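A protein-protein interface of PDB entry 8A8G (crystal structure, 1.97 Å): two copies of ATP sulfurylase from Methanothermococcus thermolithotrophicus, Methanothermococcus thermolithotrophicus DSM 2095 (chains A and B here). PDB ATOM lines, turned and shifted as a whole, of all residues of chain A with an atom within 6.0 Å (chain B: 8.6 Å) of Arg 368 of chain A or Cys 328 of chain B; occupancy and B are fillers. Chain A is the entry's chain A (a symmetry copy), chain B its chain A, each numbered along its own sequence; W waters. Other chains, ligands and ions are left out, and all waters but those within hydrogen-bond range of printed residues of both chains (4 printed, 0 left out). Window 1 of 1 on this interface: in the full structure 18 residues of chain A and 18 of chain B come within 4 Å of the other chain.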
ATOM      1  N   PRO A 198     -14.570  26.102  -3.599  1.00  0.00           N
ATOM      2  CA  PRO A 198     -15.699  25.229  -3.277  1.00  0.00           C
ATOM      3  C   PRO A 198     -16.829  25.993  -2.619  1.00  0.00           C
ATOM      4  O   PRO A 198     -16.606  26.773  -1.693  1.00  0.00           O
ATOM      5  CB  PRO A 198     -15.089  24.216  -2.305  1.00  0.00           C
ATOM      6  CG  PRO A 198     -14.024  24.977  -1.637  1.00  0.00           C
ATOM      7  CD  PRO A 198     -13.429  25.862  -2.698  1.00  0.00           C
ATOM      8  N   LEU A 200     -21.088  25.129  -1.096  1.00  0.00           N
ATOM      9  CA  LEU A 200     -21.707  23.944  -0.442  1.00  0.00           C
ATOM     10  C   LEU A 200     -22.159  22.906  -1.476  1.00  0.00           C
ATOM     11  O   LEU A 200     -22.010  21.701  -1.191  1.00  0.00           O
ATOM     12  CB  LEU A 200     -22.833  24.379   0.495  1.00  0.00           C
ATOM     13  CG  LEU A 200     -22.469  24.242   1.971  1.00  0.00           C
ATOM     14  CD1 LEU A 200     -21.579  25.390   2.419  1.00  0.00           C
ATOM     15  CD2 LEU A 200     -23.720  24.168   2.833  1.00  0.00           C
ATOM     16  N   GLU A 203     -19.329  20.504  -2.184  1.00  0.00           N
ATOM     17  CA  GLU A 203     -19.163  19.605  -1.049  1.00  0.00           C
ATOM     18  C   GLU A 203     -20.272  18.570  -0.995  1.00  0.00           C
ATOM     19  O   GLU A 203     -20.019  17.400  -0.721  1.00  0.00           O
ATOM     20  CB  GLU A 203     -19.120  20.442   0.222  1.00  0.00           C
ATOM     21  CG  GLU A 203     -18.861  19.694   1.505  1.00  0.00           C
ATOM     22  CD  GLU A 203     -18.829  20.651   2.691  1.00  0.00           C
ATOM     23  OE1 GLU A 203     -18.735  21.890   2.442  1.00  0.00           O
ATOM     24  OE2 GLU A 203     -18.893  20.179   3.844  1.00  0.00           O
ATOM     25  N   LYS A 207     -19.341  14.575  -1.014  1.00  0.00           N
ATOM     26  CA  LYS A 207     -19.674  13.722   0.121  1.00  0.00           C
ATOM     27  C   LYS A 207     -20.811  12.766  -0.201  1.00  0.00           C
ATOM     28  O   LYS A 207     -20.945  11.717   0.435  1.00  0.00           O
ATOM     29  CB  LYS A 207     -20.034  14.573   1.340  1.00  0.00           C
ATOM     30  CG  LYS A 207     -18.849  15.389   1.875  1.00  0.00           C
ATOM     31  CD  LYS A 207     -19.194  16.192   3.114  1.00  0.00           C
ATOM     32  CE  LYS A 207     -17.951  16.742   3.780  1.00  0.00           C
ATOM     33  NZ  LYS A 207     -18.345  17.561   4.952  1.00  0.00           N
ATOM     34  N   LEU A 242     -11.206  23.853   3.310  1.00  0.00           N
ATOM     35  CA  LEU A 242     -12.395  23.014   3.327  1.00  0.00           C
ATOM     36  C   LEU A 242     -12.084  21.630   3.878  1.00  0.00           C
ATOM     37  O   LEU A 242     -12.767  21.137   4.782  1.00  0.00           O
ATOM     38  CB  LEU A 242     -12.960  22.902   1.920  1.00  0.00           C
ATOM     39  CG  LEU A 242     -14.210  22.047   1.850  1.00  0.00           C
ATOM     40  CD1 LEU A 242     -15.376  22.765   2.470  1.00  0.00           C
ATOM     41  CD2 LEU A 242     -14.473  21.717   0.412  1.00  0.00           C
ATOM     42  N   TYR A 246     -13.815  20.273   7.254  1.00  0.00           N
ATOM     43  CA  TYR A 246     -15.075  19.598   7.013  1.00  0.00           C
ATOM     44  C   TYR A 246     -14.974  18.186   6.466  1.00  0.00           C
ATOM     45  O   TYR A 246     -16.005  17.540   6.297  1.00  0.00           O
ATOM     46  CB  TYR A 246     -15.907  20.458   6.058  1.00  0.00           C
ATOM     47  CG  TYR A 246     -16.330  21.740   6.711  1.00  0.00           C
ATOM     48  CD1 TYR A 246     -15.532  22.866   6.660  1.00  0.00           C
ATOM     49  CD2 TYR A 246     -17.538  21.826   7.394  1.00  0.00           C
ATOM     50  CE1 TYR A 246     -15.918  24.059   7.288  1.00  0.00           C
ATOM     51  CE2 TYR A 246     -17.941  23.020   8.009  1.00  0.00           C
ATOM     52  CZ  TYR A 246     -17.112  24.114   7.972  1.00  0.00           C
ATOM     53  OH  TYR A 246     -17.502  25.296   8.556  1.00  0.00           O
ATOM     54  N   PRO A 363     -23.730  34.071   2.254  1.00  0.00           N
ATOM     55  CA  PRO A 363     -24.330  33.272   3.313  1.00  0.00           C
ATOM     56  C   PRO A 363     -23.609  31.942   3.456  1.00  0.00           C
ATOM     57  O   PRO A 363     -23.044  31.406   2.499  1.00  0.00           O
ATOM     58  CB  PRO A 363     -25.767  33.077   2.823  1.00  0.00           C
ATOM     59  CG  PRO A 363     -25.984  34.113   1.816  1.00  0.00           C
ATOM     60  CD  PRO A 363     -24.675  34.338   1.162  1.00  0.00           C
ATOM     61  N   GLU A 364     -23.668  31.387   4.661  1.00  0.00           N
ATOM     62  CA  GLU A 364     -22.973  30.143   4.959  1.00  0.00           C
ATOM     63  C   GLU A 364     -23.681  28.912   4.402  1.00  0.00           C
ATOM     64  O   GLU A 364     -23.128  27.809   4.502  1.00  0.00           O
ATOM     65  CB  GLU A 364     -22.795  30.000   6.476  1.00  0.00           C
ATOM     66  CG  GLU A 364     -21.818  31.007   7.052  1.00  0.00           C
ATOM     67  CD  GLU A 364     -21.612  30.850   8.542  1.00  0.00           C
ATOM     68  OE1 GLU A 364     -21.399  29.683   8.987  1.00  0.00           O
ATOM     69  OE2 GLU A 364     -21.668  31.907   9.262  1.00  0.00           O
ATOM     70  N   PHE A 366     -24.145  29.006   1.272  1.00  0.00           N
ATOM     71  CA  PHE A 366     -23.358  29.034   0.046  1.00  0.00           C
ATOM     72  C   PHE A 366     -21.877  28.730   0.274  1.00  0.00           C
ATOM     73  O   PHE A 366     -21.231  28.127  -0.586  1.00  0.00           O
ATOM     74  CB  PHE A 366     -23.431  30.419  -0.608  1.00  0.00           C
ATOM     75  CG  PHE A 366     -24.655  30.679  -1.425  1.00  0.00           C
ATOM     76  CD1 PHE A 366     -25.513  29.653  -1.798  1.00  0.00           C
ATOM     77  CD2 PHE A 366     -24.920  31.969  -1.846  1.00  0.00           C
ATOM     78  CE1 PHE A 366     -26.620  29.915  -2.591  1.00  0.00           C
ATOM     79  CE2 PHE A 366     -26.016  32.235  -2.617  1.00  0.00           C
ATOM     80  CZ  PHE A 366     -26.876  31.204  -2.994  1.00  0.00           C
ATOM     81  N   MET A 367     -21.303  29.187   1.384  1.00  0.00           N
ATOM     82  CA  MET A 367     -19.857  29.124   1.542  1.00  0.00           C
ATOM     83  C   MET A 367     -19.470  28.984   3.009  1.00  0.00           C
ATOM     84  O   MET A 367     -19.901  29.766   3.867  1.00  0.00           O
ATOM     85  CB  MET A 367     -19.169  30.376   0.955  1.00  0.00           C
ATOM     86  CG  MET A 367     -17.638  30.355   1.094  1.00  0.00           C
ATOM     87  SD  MET A 367     -16.758  31.641   0.216  1.00  0.00           S
ATOM     88  CE  MET A 367     -16.879  31.059  -1.463  1.00  0.00           C
ATOM     89  N   ARG A 368     -18.680  27.944   3.291  1.00  0.00           N
ATOM     90  CA  ARG A 368     -18.206  27.665   4.672  1.00  0.00           C
ATOM     91  C   ARG A 368     -17.465  28.901   5.188  1.00  0.00           C
ATOM     92  O   ARG A 368     -16.624  29.434   4.429  1.00  0.00           O
ATOM     93  CB  ARG A 368     -17.300  26.431   4.688  1.00  0.00           C
ATOM     94  CG  ARG A 368     -17.984  25.150   4.230  1.00  0.00           C
ATOM     95  CD  ARG A 368     -19.128  24.750   5.141  1.00  0.00           C
ATOM     96  NE  ARG A 368     -19.496  23.350   4.985  1.00  0.00           N
ATOM     97  CZ  ARG A 368     -20.532  22.772   5.584  1.00  0.00           C
ATOM     98  NH1 ARG A 368     -21.311  23.479   6.384  1.00  0.00           N
ATOM     99  NH2 ARG A 368     -20.784  21.493   5.380  1.00  0.00           N
ATOM    100  N   LYS A 369     -17.785  29.327   6.417  1.00  0.00           N
ATOM    101  CA  LYS A 369     -17.179  30.488   7.047  1.00  0.00           C
ATOM    102  C   LYS A 369     -15.669  30.497   6.863  1.00  0.00           C
ATOM    103  O   LYS A 369     -15.075  31.509   6.473  1.00  0.00           O
ATOM    104  CB  LYS A 369     -17.540  30.475   8.526  1.00  0.00           C
ATOM    105  CG  LYS A 369     -16.979  31.647   9.286  1.00  0.00           C
ATOM    106  CD  LYS A 369     -17.130  31.472  10.789  1.00  0.00           C
ATOM    107  CE  LYS A 369     -16.269  32.510  11.545  1.00  0.00           C
ATOM    108  NZ  LYS A 369     -15.019  31.994  12.243  1.00  0.00           N
ATOM    109  N   GLU A 370     -15.038  29.363   7.139  1.00  0.00           N
ATOM    110  CA  GLU A 370     -13.589  29.264   7.109  1.00  0.00           C
ATOM    111  C   GLU A 370     -13.049  29.376   5.697  1.00  0.00           C
ATOM    112  O   GLU A 370     -11.925  29.847   5.496  1.00  0.00           O
ATOM    113  CB  GLU A 370     -13.165  27.926   7.721  1.00  0.00           C
ATOM    114  CG  GLU A 370     -13.358  27.835   9.216  1.00  0.00           C
ATOM    115  CD  GLU A 370     -14.728  27.341   9.622  1.00  0.00           C
ATOM    116  OE1 GLU A 370     -15.532  26.953   8.733  1.00  0.00           O
ATOM    117  OE2 GLU A 370     -14.989  27.332  10.843  1.00  0.00           O
ATOM    118  N   VAL A 371     -13.809  28.901   4.717  1.00  0.00           N
ATOM    119  CA  VAL A 371     -13.414  29.072   3.328  1.00  0.00           C
ATOM    120  C   VAL A 371     -13.473  30.539   2.949  1.00  0.00           C
ATOM    121  O   VAL A 371     -12.543  31.063   2.327  1.00  0.00           O
ATOM    122  CB  VAL A 371     -14.309  28.206   2.428  1.00  0.00           C
ATOM    123  CG1 VAL A 371     -14.121  28.553   0.976  1.00  0.00           C
ATOM    124  CG2 VAL A 371     -14.004  26.743   2.645  1.00  0.00           C
ATOM    125  N   TYR A 372     -14.540  31.240   3.335  1.00  0.00           N
ATOM    126  CA  TYR A 372     -14.574  32.665   3.053  1.00  0.00           C
ATOM    127  C   TYR A 372     -13.375  33.363   3.680  1.00  0.00           C
ATOM    128  O   TYR A 372     -12.747  34.211   3.040  1.00  0.00           O
ATOM    129  CB  TYR A 372     -15.866  33.316   3.547  1.00  0.00           C
ATOM    130  CG  TYR A 372     -15.820  34.789   3.292  1.00  0.00           C
ATOM    131  CD1 TYR A 372     -15.952  35.294   2.005  1.00  0.00           C
ATOM    132  CD2 TYR A 372     -15.574  35.685   4.321  1.00  0.00           C
ATOM    133  CE1 TYR A 372     -15.855  36.666   1.753  1.00  0.00           C
ATOM    134  CE2 TYR A 372     -15.492  37.070   4.087  1.00  0.00           C
ATOM    135  CZ  TYR A 372     -15.625  37.553   2.806  1.00  0.00           C
ATOM    136  OH  TYR A 372     -15.540  38.917   2.565  1.00  0.00           O
ATOM    137  N   GLU A 373     -13.037  33.021   4.932  1.00  0.00           N
ATOM    138  CA  GLU A 373     -11.954  33.724   5.626  1.00  0.00           C
ATOM    139  C   GLU A 373     -10.620  33.477   4.963  1.00  0.00           C
ATOM    140  O   GLU A 373      -9.746  34.346   4.978  1.00  0.00           O
ATOM    141  CB  GLU A 373     -11.900  33.301   7.083  1.00  0.00           C
ATOM    142  CG  GLU A 373     -13.148  33.706   7.864  1.00  0.00           C
ATOM    143  CD  GLU A 373     -13.172  33.157   9.278  1.00  0.00           C
ATOM    144  OE1 GLU A 373     -12.691  32.003   9.504  1.00  0.00           O
ATOM    145  OE2 GLU A 373     -13.668  33.893  10.174  1.00  0.00           O
ATOM    146  N   TYR B 323     -26.792  11.864  12.507  1.00  0.00           N
ATOM    147  CA  TYR B 323     -26.941  12.837  13.614  1.00  0.00           C
ATOM    148  C   TYR B 323     -26.831  14.245  13.042  1.00  0.00           C
ATOM    149  O   TYR B 323     -26.238  14.404  11.965  1.00  0.00           O
ATOM    150  CB  TYR B 323     -25.838  12.614  14.648  1.00  0.00           C
ATOM    151  CG  TYR B 323     -24.443  12.650  14.079  1.00  0.00           C
ATOM    152  CD1 TYR B 323     -23.779  13.849  13.887  1.00  0.00           C
ATOM    153  CD2 TYR B 323     -23.787  11.485  13.723  1.00  0.00           C
ATOM    154  CE1 TYR B 323     -22.499  13.891  13.363  1.00  0.00           C
ATOM    155  CE2 TYR B 323     -22.506  11.509  13.197  1.00  0.00           C
ATOM    156  CZ  TYR B 323     -21.859  12.716  13.016  1.00  0.00           C
ATOM    157  OH  TYR B 323     -20.598  12.746  12.499  1.00  0.00           O
ATOM    158  N   TYR B 324     -27.442  15.218  13.710  1.00  0.00           N
ATOM    159  CA  TYR B 324     -27.282  16.609  13.231  1.00  0.00           C
ATOM    160  C   TYR B 324     -25.900  17.092  13.670  1.00  0.00           C
ATOM    161  O   TYR B 324     -25.501  16.814  14.813  1.00  0.00           O
ATOM    162  CB  TYR B 324     -28.368  17.536  13.775  1.00  0.00           C
ATOM    163  CG  TYR B 324     -28.244  18.936  13.236  1.00  0.00           C
ATOM    164  CD1 TYR B 324     -28.789  19.274  12.010  1.00  0.00           C
ATOM    165  CD2 TYR B 324     -27.538  19.907  13.922  1.00  0.00           C
ATOM    166  CE1 TYR B 324     -28.663  20.551  11.494  1.00  0.00           C
ATOM    167  CE2 TYR B 324     -27.402  21.189  13.420  1.00  0.00           C
ATOM    168  CZ  TYR B 324     -27.966  21.512  12.200  1.00  0.00           C
ATOM    169  OH  TYR B 324     -27.840  22.771  11.695  1.00  0.00           O
ATOM    170  N   CYS B 325     -25.187  17.778  12.781  1.00  0.00           N
ATOM    171  CA  CYS B 325     -23.853  18.305  13.154  1.00  0.00           C
ATOM    172  C   CYS B 325     -23.918  19.831  13.170  1.00  0.00           C
ATOM    173  O   CYS B 325     -24.321  20.414  12.155  1.00  0.00           O
ATOM    174  CB  CYS B 325     -22.776  17.856  12.183  1.00  0.00           C
ATOM    175  SG  CYS B 325     -21.183  18.611  12.579  1.00  0.00           S
ATOM    176  N   LYS B 326     -23.494  20.439  14.275  1.00  0.00           N
ATOM    177  CA  LYS B 326     -23.600  21.879  14.420  1.00  0.00           C
ATOM    178  C   LYS B 326     -22.443  22.635  13.803  1.00  0.00           C
ATOM    179  O   LYS B 326     -22.415  23.865  13.911  1.00  0.00           O
ATOM    180  CB  LYS B 326     -23.696  22.244  15.900  1.00  0.00           C
ATOM    181  CG  LYS B 326     -24.977  21.718  16.523  1.00  0.00           C
ATOM    182  CD  LYS B 326     -25.112  22.113  17.975  1.00  0.00           C
ATOM    183  CE  LYS B 326     -24.317  21.180  18.877  1.00  0.00           C
ATOM    184  NZ  LYS B 326     -24.703  21.423  20.328  1.00  0.00           N
ATOM    185  N   LYS B 327     -21.476  21.954  13.195  1.00  0.00           N
ATOM    186  CA  LYS B 327     -20.514  22.633  12.333  1.00  0.00           C
ATOM    187  C   LYS B 327     -20.770  22.366  10.855  1.00  0.00           C
ATOM    188  O   LYS B 327     -20.720  23.295  10.038  1.00  0.00           O
ATOM    189  CB  LYS B 327     -19.096  22.218  12.707  1.00  0.00           C
ATOM    190  CG  LYS B 327     -18.066  22.789  11.783  1.00  0.00           C
ATOM    191  CD  LYS B 327     -16.694  22.778  12.440  1.00  0.00           C
ATOM    192  CE  LYS B 327     -15.665  23.442  11.542  1.00  0.00           C
ATOM    193  NZ  LYS B 327     -14.413  23.733  12.325  1.00  0.00           N
ATOM    194  N   CYS B 328     -21.087  21.127  10.480  1.00  0.00           N
ATOM    195  CA  CYS B 328     -21.564  20.883   9.128  1.00  0.00           C
ATOM    196  C   CYS B 328     -22.894  21.585   8.896  1.00  0.00           C
ATOM    197  O   CYS B 328     -23.224  21.932   7.762  1.00  0.00           O
ATOM    198  CB  CYS B 328     -21.674  19.385   8.867  1.00  0.00           C
ATOM    199  SG  CYS B 328     -20.073  18.471   8.831  1.00  0.00           S
ATOM    200  N   ASN B 329     -23.670  21.826   9.962  1.00  0.00           N
ATOM    201  CA  ASN B 329     -25.002  22.448   9.862  1.00  0.00           C
ATOM    202  C   ASN B 329     -25.964  21.586   9.037  1.00  0.00           C
ATOM    203  O   ASN B 329     -26.694  22.060   8.171  1.00  0.00           O
ATOM    204  CB  ASN B 329     -24.906  23.858   9.277  1.00  0.00           C
ATOM    205  CG  ASN B 329     -24.094  24.799  10.158  1.00  0.00           C
ATOM    206  OD1 ASN B 329     -24.035  24.630  11.380  1.00  0.00           O
ATOM    207  ND2 ASN B 329     -23.449  25.793   9.534  1.00  0.00           N
ATOM    208  N   ALA B 330     -25.980  20.299   9.327  1.00  0.00           N
ATOM    209  CA  ALA B 330     -26.701  19.372   8.472  1.00  0.00           C
ATOM    210  C   ALA B 330     -26.802  18.030   9.178  1.00  0.00           C
ATOM    211  O   ALA B 330     -26.036  17.723  10.090  1.00  0.00           O
ATOM    212  CB  ALA B 330     -26.010  19.242   7.117  1.00  0.00           C
ATOM    213  N   ILE B 331     -27.821  17.263   8.790  1.00  0.00           N
ATOM    214  CA  ILE B 331     -27.876  15.862   9.202  1.00  0.00           C
ATOM    215  C   ILE B 331     -26.812  15.124   8.411  1.00  0.00           C
ATOM    216  O   ILE B 331     -26.791  15.171   7.173  1.00  0.00           O
ATOM    217  CB  ILE B 331     -29.268  15.277   8.958  1.00  0.00           C
ATOM    218  CG1 ILE B 331     -30.298  15.998   9.824  1.00  0.00           C
ATOM    219  CG2 ILE B 331     -29.291  13.772   9.238  1.00  0.00           C
ATOM    220  CD1 ILE B 331     -31.665  15.354   9.794  1.00  0.00           C
ATOM    221  N   VAL B 332     -25.907  14.459   9.113  1.00  0.00           N
ATOM    222  CA  VAL B 332     -24.758  13.841   8.469  1.00  0.00           C
ATOM    223  C   VAL B 332     -24.550  12.462   9.068  1.00  0.00           C
ATOM    224  O   VAL B 332     -25.359  12.002   9.874  1.00  0.00           O
ATOM    225  CB  VAL B 332     -23.505  14.715   8.639  1.00  0.00           C
ATOM    226  CG1 VAL B 332     -23.687  16.017   7.945  1.00  0.00           C
ATOM    227  CG2 VAL B 332     -23.252  14.933  10.088  1.00  0.00           C
ATOM    228  N   HIS B 333     -23.446  11.820   8.680  1.00  0.00           N
ATOM    229  CA  HIS B 333     -23.041  10.506   9.251  1.00  0.00           C
ATOM    230  C   HIS B 333     -21.526  10.521   9.494  1.00  0.00           C
ATOM    231  O   HIS B 333     -20.856  11.423   8.967  1.00  0.00           O
ATOM    232  CB  HIS B 333     -23.590   9.311   8.455  1.00  0.00           C
ATOM    233  CG  HIS B 333     -23.454   9.416   6.975  1.00  0.00           C
ATOM    234  ND1 HIS B 333     -22.527   8.683   6.269  1.00  0.00           N
ATOM    235  CD2 HIS B 333     -24.137  10.141   6.065  1.00  0.00           C
ATOM    236  CE1 HIS B 333     -22.634   8.960   4.988  1.00  0.00           C
ATOM    237  NE2 HIS B 333     -23.612   9.854   4.837  1.00  0.00           N
ATOM    238  N   ILE B 336     -18.825  10.987   6.578  1.00  0.00           N
ATOM    239  CA  ILE B 336     -18.607  12.266   5.887  1.00  0.00           C
ATOM    240  C   ILE B 336     -18.405  13.444   6.838  1.00  0.00           C
ATOM    241  O   ILE B 336     -18.247  14.572   6.368  1.00  0.00           O
ATOM    242  CB  ILE B 336     -19.762  12.601   4.917  1.00  0.00           C
ATOM    243  CG1 ILE B 336     -21.079  12.678   5.686  1.00  0.00           C
ATOM    244  CG2 ILE B 336     -19.816  11.614   3.758  1.00  0.00           C
ATOM    245  CD1 ILE B 336     -22.185  13.273   4.843  1.00  0.00           C
ATOM    246  N   CYS B 337     -18.441  13.232   8.144  1.00  0.00           N
ATOM    247  CA  CYS B 337     -18.273  14.281   9.115  1.00  0.00           C
ATOM    248  C   CYS B 337     -17.141  13.911  10.058  1.00  0.00           C
ATOM    249  O   CYS B 337     -17.123  12.815  10.605  1.00  0.00           O
ATOM    250  CB  CYS B 337     -19.568  14.482   9.932  1.00  0.00           C
ATOM    251  SG  CYS B 337     -19.370  15.497  11.373  1.00  0.00           S
ATOM    252  N   PRO B 338     -16.135  14.790  10.197  1.00  0.00           N
ATOM    253  CA  PRO B 338     -14.986  14.479  11.075  1.00  0.00           C
ATOM    254  C   PRO B 338     -15.042  15.132  12.441  1.00  0.00           C
ATOM    255  O   PRO B 338     -14.033  15.063  13.158  1.00  0.00           O
ATOM    256  CB  PRO B 338     -13.843  15.083  10.257  1.00  0.00           C
ATOM    257  CG  PRO B 338     -14.462  16.345   9.757  1.00  0.00           C
ATOM    258  CD  PRO B 338     -15.890  16.021   9.437  1.00  0.00           C
ATOM    259  N   HIS B 339     -16.157  15.749  12.814  1.00  0.00           N
ATOM    260  CA  HIS B 339     -16.215  16.614  13.977  1.00  0.00           C
ATOM    261  C   HIS B 339     -16.475  15.862  15.262  1.00  0.00           C
ATOM    262  O   HIS B 339     -17.095  14.795  15.288  1.00  0.00           O
ATOM    263  CB  HIS B 339     -17.284  17.676  13.774  1.00  0.00           C
ATOM    264  CG  HIS B 339     -17.049  18.510  12.568  1.00  0.00           C
ATOM    265  ND1 HIS B 339     -17.998  18.690  11.592  1.00  0.00           N
ATOM    266  CD2 HIS B 339     -15.961  19.211  12.178  1.00  0.00           C
ATOM    267  CE1 HIS B 339     -17.500  19.468  10.646  1.00  0.00           C
ATOM    268  NE2 HIS B 339     -16.267  19.804  10.985  1.00  0.00           N
ATOM    269  N   TYR B 343     -20.187  18.804  18.730  1.00  0.00           N
ATOM    270  CA  TYR B 343     -20.920  19.284  17.573  1.00  0.00           C
ATOM    271  C   TYR B 343     -22.055  18.360  17.165  1.00  0.00           C
ATOM    272  O   TYR B 343     -22.879  18.774  16.354  1.00  0.00           O
ATOM    273  CB  TYR B 343     -19.958  19.460  16.397  1.00  0.00           C
ATOM    274  CG  TYR B 343     -18.921  20.534  16.623  1.00  0.00           C
ATOM    275  CD1 TYR B 343     -19.234  21.869  16.469  1.00  0.00           C
ATOM    276  CD2 TYR B 343     -17.634  20.213  16.990  1.00  0.00           C
ATOM    277  CE1 TYR B 343     -18.287  22.844  16.685  1.00  0.00           C
ATOM    278  CE2 TYR B 343     -16.674  21.188  17.190  1.00  0.00           C
ATOM    279  CZ  TYR B 343     -17.012  22.494  17.059  1.00  0.00           C
ATOM    280  OH  TYR B 343     -16.070  23.460  17.266  1.00  0.00           O
ATOM    281  N   ARG B 344     -22.122  17.145  17.702  1.00  0.00           N
ATOM    282  CA  ARG B 344     -23.054  16.120  17.275  1.00  0.00           C
ATOM    283  C   ARG B 344     -24.279  16.104  18.165  1.00  0.00           C
ATOM    284  O   ARG B 344     -24.168  16.114  19.395  1.00  0.00           O
ATOM    285  CB  ARG B 344     -22.411  14.734  17.293  1.00  0.00           C
ATOM    286  CG  ARG B 344     -21.134  14.674  16.507  1.00  0.00           C
ATOM    287  CD  ARG B 344     -20.665  13.250  16.208  1.00  0.00           C
ATOM    288  NE  ARG B 344     -19.467  13.311  15.372  1.00  0.00           N
ATOM    289  CZ  ARG B 344     -18.897  12.274  14.764  1.00  0.00           C
ATOM    290  NH1 ARG B 344     -19.361  11.040  14.908  1.00  0.00           N
ATOM    291  NH2 ARG B 344     -17.841  12.481  13.978  1.00  0.00           N
HETATM  292  O   HOH W   1     -19.754  25.861  10.089  1.00  0.00           O
HETATM  293  O   HOH W   2     -20.327  16.613   6.465  1.00  0.00           O
HETATM  294  O   HOH W   3     -24.772  25.891   6.631  1.00  0.00           O
HETATM  295  O   HOH W   4     -23.175  20.068   5.225  1.00  0.00           O
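OE2 of Glu 370 of chain A is in salt-bridge range of NZ of Lys 327 of chain B, at 3.9 Å. The backbone carbonyl oxygen (O) of Cys 328 of chain B lies within hydrogen-bond range of the guanidinium group (NH1) of Arg 368 of chain A (2.8 Å). O of Ile 336 of chain B is in hydrogen-bond range of NZ of Lys 207 of chain A, 3.3 Å away.
SG of Cys 325 of chain B sits close to N of Lys 327 of chain B (3.4 Å). The side-chain amino group (NZ) of Lys 207 of chain A is in salt-bridge range of the side-chain carboxylate (OE2) of Glu 203 of chain A (2.9 Å). NH2 of Arg 368 of chain A lies within salt-bridge range of OE2 of Glu 203 of chain A. O of Tyr 246 of chain A lies within hydrogen-bond range of NZ of Lys 207 of chain A, at 2.7 Å. The side-chain hydroxyl of Tyr 246 of chain A lies within hydrogen-bond range of the side-chain carboxylate of Glu 370 of chain A (2.6 Å).
Among the printed residues, merely in contact across the chains: Tyr 246 of chain A with Lys 327 of chain B (3.5 Å), Tyr 246 of chain A with Pro 338 of chain B (3.5 Å), Arg 368 of chain A with Lys 327 of chain B (3.7 Å) and Tyr 246 of chain A with Ile 336 of chain B (3.7 Å).
Of chain B, only Lys 327 (3.7 Å) and Cys 328 (2.8 Å) come within 4 Å of Arg 368 of chain A. Of chain A, only Arg 368 comes within 4 Å of Cys 328 of chain B. Printed residues of chain A within 4 Å of Lys 327 of chain B: Tyr 246 (3.5 Å), Arg 368 (3.7 Å) and Glu 370 (3.9 Å). Printed residues of chain A within 4 Å of Pro 338 of chain B: Tyr 246 (3.5 Å). Of the printed residues of chain B, Glu 370 of chain A touches Lys 327. Printed residues of chain B within 4 Å of Lys 207 of chain A: Ile 336 (3.3 Å). Tyr 323 of chain B touches none of the printed residues of chain A. The nearest printed residue of chain B that does not touch Tyr 246 of chain A is His 339 of chain B (4.02 Å).
Along chain A the printed residues that touch a printed residue of chain B span positions 207 to 370. Of the 17 printed residues of chain B, 4 touch a printed residue of chain A. Among the printed residues, Asp or Glu carboxylates within 4 Å of a Lys or Arg side-chain nitrogen of the other chain: Glu 370 of chain A with Lys 327 of chain B (3.9 Å).
No position is printed for both chains. Of the 7 pairs that touch across the chains among the printed residues, none has its exchanged pair printed and touching as well.
Water W2 bridges NZ of Lys 207 of chain A and O of Ile 336 of chain B. Water W1 lies within hydrogen-bond range of O of Lys 327 of chain B (2.7 Å) and OH of Tyr 246 of chain A (2.8 Å). Water W4 bridges the guanidinium group of Arg 368 of chain A (2.8 Å) and the backbone carbonyl oxygen of Cys 328 of chain B (3.1 Å). Water W3 bridges the side-chain amide nitrogen (ND2) of Asn 329 of chain B and the backbone carbonyl oxygen (O) of Glu 364 of chain A.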
